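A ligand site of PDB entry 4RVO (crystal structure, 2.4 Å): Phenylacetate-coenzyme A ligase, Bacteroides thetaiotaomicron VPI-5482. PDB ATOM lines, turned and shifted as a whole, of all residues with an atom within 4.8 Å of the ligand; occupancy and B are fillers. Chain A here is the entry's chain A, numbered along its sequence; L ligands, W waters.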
ATOM      1  N   PHE A 142      -1.643  -3.911  -2.100  1.00  0.00           N
ATOM      2  CA  PHE A 142      -1.277  -5.269  -1.662  1.00  0.00           C
ATOM      3  C   PHE A 142       0.014  -5.245  -0.858  1.00  0.00           C
ATOM      4  O   PHE A 142       1.032  -4.741  -1.337  1.00  0.00           O
ATOM      5  CB  PHE A 142      -1.128  -6.204  -2.861  1.00  0.00           C
ATOM      6  CG  PHE A 142      -2.391  -6.417  -3.649  1.00  0.00           C
ATOM      7  CD1 PHE A 142      -3.347  -7.338  -3.233  1.00  0.00           C
ATOM      8  CD2 PHE A 142      -2.576  -5.806  -4.884  1.00  0.00           C
ATOM      9  CE1 PHE A 142      -4.485  -7.576  -3.990  1.00  0.00           C
ATOM     10  CE2 PHE A 142      -3.713  -6.057  -5.648  1.00  0.00           C
ATOM     11  CZ  PHE A 142      -4.652  -6.950  -5.206  1.00  0.00           C
ATOM     12  N   THR A 143      -0.032  -5.765   0.379  1.00  0.00           N
ATOM     13  CA  THR A 143       1.106  -5.697   1.301  1.00  0.00           C
ATOM     14  C   THR A 143       2.290  -6.562   0.821  1.00  0.00           C
ATOM     15  O   THR A 143       3.425  -6.317   1.233  1.00  0.00           O
ATOM     16  CB  THR A 143       0.669  -6.105   2.687  1.00  0.00           C
ATOM     17  OG1 THR A 143       0.095  -7.410   2.627  1.00  0.00           O
ATOM     18  CG2 THR A 143      -0.321  -5.136   3.295  1.00  0.00           C
ATOM     19  N   GLY A 144       2.015  -7.547  -0.053  1.00  0.00           N
ATOM     20  CA  GLY A 144       3.047  -8.436  -0.594  1.00  0.00           C
ATOM     21  C   GLY A 144       4.064  -7.722  -1.476  1.00  0.00           C
ATOM     22  O   GLY A 144       5.229  -8.126  -1.536  1.00  0.00           O
ATOM     23  N   ILE A 213       6.673 -18.897  -1.252  1.00  0.00           N
ATOM     24  CA  ILE A 213       5.270 -19.053  -1.678  1.00  0.00           C
ATOM     25  C   ILE A 213       4.323 -18.922  -0.469  1.00  0.00           C
ATOM     26  O   ILE A 213       4.575 -19.490   0.592  1.00  0.00           O
ATOM     27  CB  ILE A 213       5.047 -20.398  -2.442  1.00  0.00           C
ATOM     28  CG1 ILE A 213       5.355 -21.642  -1.528  1.00  0.00           C
ATOM     29  CG2 ILE A 213       5.884 -20.441  -3.743  1.00  0.00           C
ATOM     30  CD1 ILE A 213       5.060 -23.011  -2.191  1.00  0.00           C
ATOM     31  N   GLY A 214       3.215 -18.217  -0.671  1.00  0.00           N
ATOM     32  CA  GLY A 214       2.183 -18.061   0.353  1.00  0.00           C
ATOM     33  C   GLY A 214       0.900 -17.452  -0.180  1.00  0.00           C
ATOM     34  O   GLY A 214       0.558 -17.677  -1.344  1.00  0.00           O
ATOM     35  N   ALA A 215       0.175 -16.695   0.686  1.00  0.00           N
ATOM     36  CA  ALA A 215      -1.051 -15.958   0.313  1.00  0.00           C
ATOM     37  C   ALA A 215      -2.304 -16.891   0.219  1.00  0.00           C
ATOM     38  O   ALA A 215      -3.422 -16.428   0.417  1.00  0.00           O
ATOM     39  CB  ALA A 215      -0.855 -15.216  -1.005  1.00  0.00           C
ATOM     40  N   GLU A 216      -2.100 -18.176  -0.103  1.00  0.00           N
ATOM     41  CA  GLU A 216      -3.237 -19.108  -0.219  1.00  0.00           C
ATOM     42  C   GLU A 216      -2.870 -20.490   0.313  1.00  0.00           C
ATOM     43  O   GLU A 216      -1.697 -20.872   0.322  1.00  0.00           O
ATOM     44  CB  GLU A 216      -3.746 -19.201  -1.693  1.00  0.00           C
ATOM     45  CG  GLU A 216      -2.723 -19.766  -2.678  1.00  0.00           C
ATOM     46  CD  GLU A 216      -3.168 -19.723  -4.133  1.00  0.00           C
ATOM     47  OE1 GLU A 216      -4.221 -19.096  -4.427  1.00  0.00           O
ATOM     48  OE2 GLU A 216      -2.445 -20.287  -4.990  1.00  0.00           O
ATOM     49  N   PRO A 217      -3.867 -21.289   0.766  1.00  0.00           N
ATOM     50  CA  PRO A 217      -3.550 -22.611   1.301  1.00  0.00           C
ATOM     51  C   PRO A 217      -3.056 -23.548   0.218  1.00  0.00           C
ATOM     52  O   PRO A 217      -3.569 -23.540  -0.905  1.00  0.00           O
ATOM     53  CB  PRO A 217      -4.895 -23.084   1.892  1.00  0.00           C
ATOM     54  CG  PRO A 217      -5.756 -21.856   1.965  1.00  0.00           C
ATOM     55  CD  PRO A 217      -5.309 -20.992   0.855  1.00  0.00           C
ATOM     56  N   HIS A 218      -2.017 -24.333   0.542  1.00  0.00           N
ATOM     57  CA  HIS A 218      -1.446 -25.310  -0.375  1.00  0.00           C
ATOM     58  C   HIS A 218      -0.843 -26.468   0.414  1.00  0.00           C
ATOM     59  O   HIS A 218      -0.357 -26.256   1.522  1.00  0.00           O
ATOM     60  CB  HIS A 218      -0.368 -24.649  -1.270  1.00  0.00           C
ATOM     61  CG  HIS A 218       0.786 -24.073  -0.506  1.00  0.00           C
ATOM     62  ND1 HIS A 218       0.686 -22.863   0.149  1.00  0.00           N
ATOM     63  CD2 HIS A 218       2.050 -24.550  -0.363  1.00  0.00           C
ATOM     64  CE1 HIS A 218       1.872 -22.650   0.709  1.00  0.00           C
ATOM     65  NE2 HIS A 218       2.725 -23.648   0.429  1.00  0.00           N
ATOM     66  N   ASN A 236       7.263 -21.905   2.749  1.00  0.00           N
ATOM     67  CA  ASN A 236       5.938 -21.360   3.032  1.00  0.00           C
ATOM     68  C   ASN A 236       6.051 -20.012   3.733  1.00  0.00           C
ATOM     69  O   ASN A 236       6.804 -19.871   4.710  1.00  0.00           O
ATOM     70  CB  ASN A 236       5.120 -22.352   3.872  1.00  0.00           C
ATOM     71  CG  ASN A 236       3.628 -22.106   3.787  1.00  0.00           C
ATOM     72  OD1 ASN A 236       3.148 -21.154   3.155  1.00  0.00           O
ATOM     73  ND2 ASN A 236       2.840 -22.992   4.404  1.00  0.00           N
ATOM     74  N   SER A 237       5.301 -19.008   3.238  1.00  0.00           N
ATOM     75  CA  SER A 237       5.315 -17.649   3.768  1.00  0.00           C
ATOM     76  C   SER A 237       3.912 -17.235   4.209  1.00  0.00           C
ATOM     77  O   SER A 237       2.997 -17.173   3.381  1.00  0.00           O
ATOM     78  CB  SER A 237       5.839 -16.673   2.708  1.00  0.00           C
ATOM     79  OG  SER A 237       5.744 -15.317   3.123  1.00  0.00           O
ATOM     80  N   PHE A 238       3.744 -16.924   5.498  1.00  0.00           N
ATOM     81  CA  PHE A 238       2.450 -16.500   6.010  1.00  0.00           C
ATOM     82  C   PHE A 238       2.440 -15.024   6.335  1.00  0.00           C
ATOM     83  O   PHE A 238       3.460 -14.463   6.737  1.00  0.00           O
ATOM     84  CB  PHE A 238       2.053 -17.308   7.249  1.00  0.00           C
ATOM     85  CG  PHE A 238       0.734 -16.896   7.879  1.00  0.00           C
ATOM     86  CD1 PHE A 238      -0.475 -17.199   7.259  1.00  0.00           C
ATOM     87  CD2 PHE A 238       0.701 -16.297   9.127  1.00  0.00           C
ATOM     88  CE1 PHE A 238      -1.687 -16.843   7.851  1.00  0.00           C
ATOM     89  CE2 PHE A 238      -0.510 -15.941   9.719  1.00  0.00           C
ATOM     90  CZ  PHE A 238      -1.706 -16.228   9.086  1.00  0.00           C
ATOM     91  N   GLY A 239       1.281 -14.407   6.207  1.00  0.00           N
ATOM     92  CA  GLY A 239       1.085 -13.024   6.572  1.00  0.00           C
ATOM     93  C   GLY A 239      -0.309 -12.532   6.262  1.00  0.00           C
ATOM     94  O   GLY A 239      -1.073 -13.204   5.568  1.00  0.00           O
ATOM     95  N   MET A 240      -0.655 -11.382   6.807  1.00  0.00           N
ATOM     96  CA  MET A 240      -1.933 -10.738   6.520  1.00  0.00           C
ATOM     97  C   MET A 240      -1.804  -9.236   6.711  1.00  0.00           C
ATOM     98  O   MET A 240      -0.901  -8.787   7.419  1.00  0.00           O
ATOM     99  CB  MET A 240      -3.067 -11.320   7.410  1.00  0.00           C
ATOM    100  CG  MET A 240      -2.975 -10.880   8.863  1.00  0.00           C
ATOM    101  SD  MET A 240      -4.183 -11.863  10.026  1.00  0.00           S
ATOM    102  CE  MET A 240      -5.837 -11.549   9.129  1.00  0.00           C
ATOM    103  N   THR A 241      -2.637  -8.444   6.015  1.00  0.00           N
ATOM    104  CA  THR A 241      -2.558  -6.979   6.039  1.00  0.00           C
ATOM    105  C   THR A 241      -2.632  -6.440   7.482  1.00  0.00           C
ATOM    106  O   THR A 241      -1.818  -5.587   7.866  1.00  0.00           O
ATOM    107  CB  THR A 241      -3.682  -6.381   5.163  1.00  0.00           C
ATOM    108  OG1 THR A 241      -3.581  -6.939   3.838  1.00  0.00           O
ATOM    109  CG2 THR A 241      -3.609  -4.832   5.082  1.00  0.00           C
ATOM    110  N   GLU A 242      -3.566  -6.983   8.299  1.00  0.00           N
ATOM    111  CA  GLU A 242      -3.759  -6.552   9.693  1.00  0.00           C
ATOM    112  C   GLU A 242      -2.446  -6.674  10.507  1.00  0.00           C
ATOM    113  O   GLU A 242      -2.208  -5.875  11.415  1.00  0.00           O
ATOM    114  CB  GLU A 242      -4.872  -7.385  10.362  1.00  0.00           C
ATOM    115  CG  GLU A 242      -6.269  -7.119   9.805  1.00  0.00           C
ATOM    116  CD  GLU A 242      -6.633  -7.896   8.556  1.00  0.00           C
ATOM    117  OE1 GLU A 242      -5.746  -8.569   7.979  1.00  0.00           O
ATOM    118  OE2 GLU A 242      -7.829  -7.853   8.165  1.00  0.00           O
ATOM    119  N   MET A 258       5.836 -23.268  10.295  1.00  0.00           N
ATOM    120  CA  MET A 258       6.272 -21.884  10.090  1.00  0.00           C
ATOM    121  C   MET A 258       6.566 -21.203  11.412  1.00  0.00           C
ATOM    122  O   MET A 258       5.663 -21.058  12.249  1.00  0.00           O
ATOM    123  CB  MET A 258       5.221 -21.094   9.312  1.00  0.00           C
ATOM    124  CG  MET A 258       5.110 -21.488   7.862  1.00  0.00           C
ATOM    125  SD  MET A 258       3.664 -20.590   6.987  1.00  0.00           S
ATOM    126  CE  MET A 258       2.211 -21.588   7.682  1.00  0.00           C
ATOM    127  N   ASP A 305      -8.456 -17.573  10.729  1.00  0.00           N
ATOM    128  CA  ASP A 305      -7.605 -18.634  10.181  1.00  0.00           C
ATOM    129  C   ASP A 305      -7.525 -19.797  11.133  1.00  0.00           C
ATOM    130  O   ASP A 305      -7.388 -19.595  12.353  1.00  0.00           O
ATOM    131  CB  ASP A 305      -6.195 -18.104   9.893  1.00  0.00           C
ATOM    132  CG  ASP A 305      -6.134 -17.123   8.748  1.00  0.00           C
ATOM    133  OD1 ASP A 305      -6.932 -17.283   7.791  1.00  0.00           O
ATOM    134  OD2 ASP A 305      -5.224 -16.286   8.748  1.00  0.00           O
ATOM    135  N   ILE A 326      -2.018 -23.352   7.202  1.00  0.00           N
ATOM    136  CA  ILE A 326      -3.399 -22.862   7.291  1.00  0.00           C
ATOM    137  C   ILE A 326      -4.211 -23.565   6.214  1.00  0.00           C
ATOM    138  O   ILE A 326      -3.957 -23.368   5.027  1.00  0.00           O
ATOM    139  CB  ILE A 326      -3.463 -21.312   7.132  1.00  0.00           C
ATOM    140  CG1 ILE A 326      -2.274 -20.582   7.860  1.00  0.00           C
ATOM    141  CG2 ILE A 326      -4.837 -20.779   7.560  1.00  0.00           C
ATOM    142  CD1 ILE A 326      -2.288 -20.632   9.363  1.00  0.00           C
ATOM    143  N   ARG A 329     -10.635 -21.653   7.032  1.00  0.00           N
ATOM    144  CA  ARG A 329     -11.065 -20.514   7.844  1.00  0.00           C
ATOM    145  C   ARG A 329     -12.396 -20.799   8.568  1.00  0.00           C
ATOM    146  O   ARG A 329     -13.136 -21.700   8.159  1.00  0.00           O
ATOM    147  CB  ARG A 329     -11.196 -19.257   6.969  1.00  0.00           C
ATOM    148  CG  ARG A 329      -9.867 -18.608   6.658  1.00  0.00           C
ATOM    149  CD  ARG A 329     -10.019 -17.448   5.704  1.00  0.00           C
ATOM    150  NE  ARG A 329     -10.725 -16.309   6.317  1.00  0.00           N
ATOM    151  CZ  ARG A 329     -10.118 -15.265   6.867  1.00  0.00           C
ATOM    152  NH1 ARG A 329      -8.794 -15.221   6.942  1.00  0.00           N
ATOM    153  NH2 ARG A 329     -10.827 -14.260   7.353  1.00  0.00           N
ATOM    154  N   MET A 333     -15.050 -16.412   3.954  1.00  0.00           N
ATOM    155  CA  MET A 333     -14.098 -15.840   3.001  1.00  0.00           C
ATOM    156  C   MET A 333     -13.369 -16.930   2.184  1.00  0.00           C
ATOM    157  O   MET A 333     -12.940 -17.938   2.751  1.00  0.00           O
ATOM    158  CB  MET A 333     -13.088 -14.972   3.737  1.00  0.00           C
ATOM    159  CG  MET A 333     -12.383 -13.992   2.849  1.00  0.00           C
ATOM    160  SD  MET A 333     -10.783 -13.296   3.653  1.00  0.00           S
ATOM    161  CE  MET A 333      -9.626 -14.830   3.351  1.00  0.00           C
ATOM    162  N   ILE A 335     -10.205 -17.612  -1.040  1.00  0.00           N
ATOM    163  CA  ILE A 335      -9.031 -17.025  -1.668  1.00  0.00           C
ATOM    164  C   ILE A 335      -8.822 -17.600  -3.075  1.00  0.00           C
ATOM    165  O   ILE A 335      -8.686 -18.808  -3.243  1.00  0.00           O
ATOM    166  CB  ILE A 335      -7.768 -17.244  -0.778  1.00  0.00           C
ATOM    167  CG1 ILE A 335      -7.995 -16.710   0.661  1.00  0.00           C
ATOM    168  CG2 ILE A 335      -6.528 -16.617  -1.419  1.00  0.00           C
ATOM    169  CD1 ILE A 335      -6.958 -17.135   1.655  1.00  0.00           C
ATOM    170  N   GLY A 338      -4.579 -15.880  -4.794  1.00  0.00           N
ATOM    171  CA  GLY A 338      -3.939 -15.249  -3.639  1.00  0.00           C
ATOM    172  C   GLY A 338      -4.697 -14.046  -3.111  1.00  0.00           C
ATOM    173  O   GLY A 338      -4.226 -13.382  -2.179  1.00  0.00           O
ATOM    174  N   ASN A 340      -7.991 -12.347  -1.249  1.00  0.00           N
ATOM    175  CA  ASN A 340      -9.093 -12.607  -0.332  1.00  0.00           C
ATOM    176  C   ASN A 340     -10.392 -11.985  -0.830  1.00  0.00           C
ATOM    177  O   ASN A 340     -10.417 -10.778  -1.124  1.00  0.00           O
ATOM    178  CB  ASN A 340      -8.750 -12.078   1.061  1.00  0.00           C
ATOM    179  CG  ASN A 340      -7.538 -12.713   1.687  1.00  0.00           C
ATOM    180  OD1 ASN A 340      -6.808 -13.482   1.050  1.00  0.00           O
ATOM    181  ND2 ASN A 340      -7.302 -12.414   2.946  1.00  0.00           N
HETATM  182  P1  LIG L   1      -2.206 -10.932   0.979  1.00  0.00           P
HETATM  183  O1  LIG L   1      -3.141 -11.931   0.291  1.00  0.00           O
HETATM  184  O2  LIG L   1      -0.788 -11.588   1.178  1.00  0.00           O
HETATM  185  O3  LIG L   1      -2.095  -9.678   0.116  1.00  0.00           O
HETATM  186  P2  LIG L   1      -4.318 -10.624   2.967  1.00  0.00           P
HETATM  187  O4  LIG L   1      -4.439  -9.808   4.201  1.00  0.00           O
HETATM  188  O5  LIG L   1      -5.296 -10.090   1.904  1.00  0.00           O
HETATM  189  O6  LIG L   1      -2.816 -10.548   2.409  1.00  0.00           O
HETATM  190  O7  LIG L   1      -4.662 -12.127   3.294  1.00  0.00           O
HETATM  191  C1  LIG L   1      -4.090 -12.844   4.399  1.00  0.00           C
HETATM  192  C2  LIG L   1      -4.748 -14.184   4.496  1.00  0.00           C
HETATM  193  O8  LIG L   1      -4.255 -15.039   3.439  1.00  0.00           O
HETATM  194  C3  LIG L   1      -4.468 -14.949   5.779  1.00  0.00           C
HETATM  195  O9  LIG L   1      -5.348 -14.528   6.827  1.00  0.00           O
HETATM  196  C4  LIG L   1      -4.712 -16.395   5.355  1.00  0.00           C
HETATM  197  O10 LIG L   1      -6.105 -16.715   5.350  1.00  0.00           O
HETATM  198  C5  LIG L   1      -4.160 -16.378   3.908  1.00  0.00           C
HETATM  199  N1  LIG L   1      -2.763 -16.812   3.803  1.00  0.00           N
HETATM  200  C6  LIG L   1      -1.647 -16.016   3.779  1.00  0.00           C
HETATM  201  N2  LIG L   1      -0.520 -16.681   3.747  1.00  0.00           N
HETATM  202  C7  LIG L   1      -0.922 -18.011   3.737  1.00  0.00           C
HETATM  203  C8  LIG L   1      -0.203 -19.217   3.716  1.00  0.00           C
HETATM  204  N3  LIG L   1       1.137 -19.288   3.736  1.00  0.00           N
HETATM  205  N4  LIG L   1      -0.903 -20.373   3.712  1.00  0.00           N
HETATM  206  C9  LIG L   1      -2.244 -20.306   3.747  1.00  0.00           C
HETATM  207  N5  LIG L   1      -3.032 -19.227   3.776  1.00  0.00           N
HETATM  208  C10 LIG L   1      -2.300 -18.100   3.764  1.00  0.00           C
HETATM  209  O   HOH W   1      -0.278 -22.860   4.878  1.00  0.00           O
HETATM  210  O   HOH W   2      -0.104  -9.341  -1.608  1.00  0.00           O
HETATM  211  O   HOH W   3      -7.497 -12.650   6.662  1.00  0.00           O
HETATM  212  O   HOH W   4      -6.461  -7.533   2.201  1.00  0.00           O
HETATM  213  O   HOH W   5      -2.338  -7.324   1.431  1.00  0.00           O
HETATM  214  O   HOH W   6      -4.353 -10.483  -1.830  1.00  0.00           O
HETATM  215  O   HOH W   7      -6.506 -10.135   5.694  1.00  0.00           O
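A nitrogen (N3) of the ligand is in hydrogen-bond range of the backbone carbonyl oxygen (O) of Ser 237 (2.8 Å). An oxygen (O9) of the ligand lies within hydrogen-bond range of the side-chain carboxylate (OD2) of Asp 305, 2.6 Å away. O10 of the ligand is in hydrogen-bond range of NH1 of Arg 329 (3.5 Å). An oxygen (O4) of the ligand lies within hydrogen-bond range of the backbone NH of Thr 241, at 2.9 Å. ND2 of Asn 340 is in hydrogen-bond range of O7 of the ligand, 2.7 Å away. The backbone carbonyl oxygen of Gly 338 sits close to an oxygen (O1) of the ligand, 3.1 Å away. N3 of the ligand sits at hydrogen-bond distance from OD1 of Asn 236 (2.8 Å). O4 of the ligand lies within hydrogen-bond range of OG1 of Thr 241, 3.0 Å away. N2 of the ligand sits at hydrogen-bond distance from N of Ala 215 (3.1 Å).
N of Gly 338 lies within hydrogen-bond range of OE1 of Glu 216. The backbone NH (N) of Ser 237 lies within hydrogen-bond range of the backbone carbonyl oxygen (O) of Ile 213, at 2.8 Å. The guanidinium group (NH1) of Arg 329 is in salt-bridge range of the side-chain carboxylate (OD1) of Asp 305. OD1 of Asn 236 lies close to O of Ile 213 (3.4 Å). O of Glu 216 sits at hydrogen-bond distance from ND1 of His 218 (3.1 Å). The side-chain sulfur (SD) of Met 258 sits close to the side-chain amide nitrogen (ND2) of Asn 236 (3.6 Å). The side-chain sulfur (SD) of Met 333 lies close to the side-chain amide nitrogen (ND2) of Asn 340 (3.7 Å).
Merely in contact with the ligand: Gly 239 (3.3 Å), Glu 216 (3.5 Å), Met 240 (3.5 Å), Pro 217 (3.5 Å), Phe 238 (3.6 Å), Ile 335 (3.7 Å), Ile 326 (3.7 Å) and Gly 214 (3.7 Å). Hydrophobic or aromatic side chains that line the ligand: Phe 238, Met 240, Ile 326 and Ile 335. The nearest printed residue that does not touch the ligand is Thr 143 (4.03 Å).
Water W2 bridges an oxygen (O3) of the ligand (2.7 Å) and the backbone NH (N) of Gly 144 (3.2 Å). Water W5 lies within hydrogen-bond range of O3 of the ligand (2.7 Å), OG1 of Thr 143 (2.7 Å) and OG1 of Thr 241 (2.7 Å). Water W1 lies within hydrogen-bond range of N4 of the ligand (2.8 Å), N of Ile 326 (2.9 Å) and ND2 of Asn 236 (3.2 Å). Water W4 bridges an oxygen (O5) of the ligand (2.8 Å) and the side-chain hydroxyl of Thr 241 (3.4 Å). Water W6 lies within hydrogen-bond range of O1 of the ligand (2.8 Å) and O of Gly 338 (2.9 Å). Water W3 lies within hydrogen-bond range of O9 of the ligand (2.9 Å) and NH1 of Arg 329 (2.9 Å).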
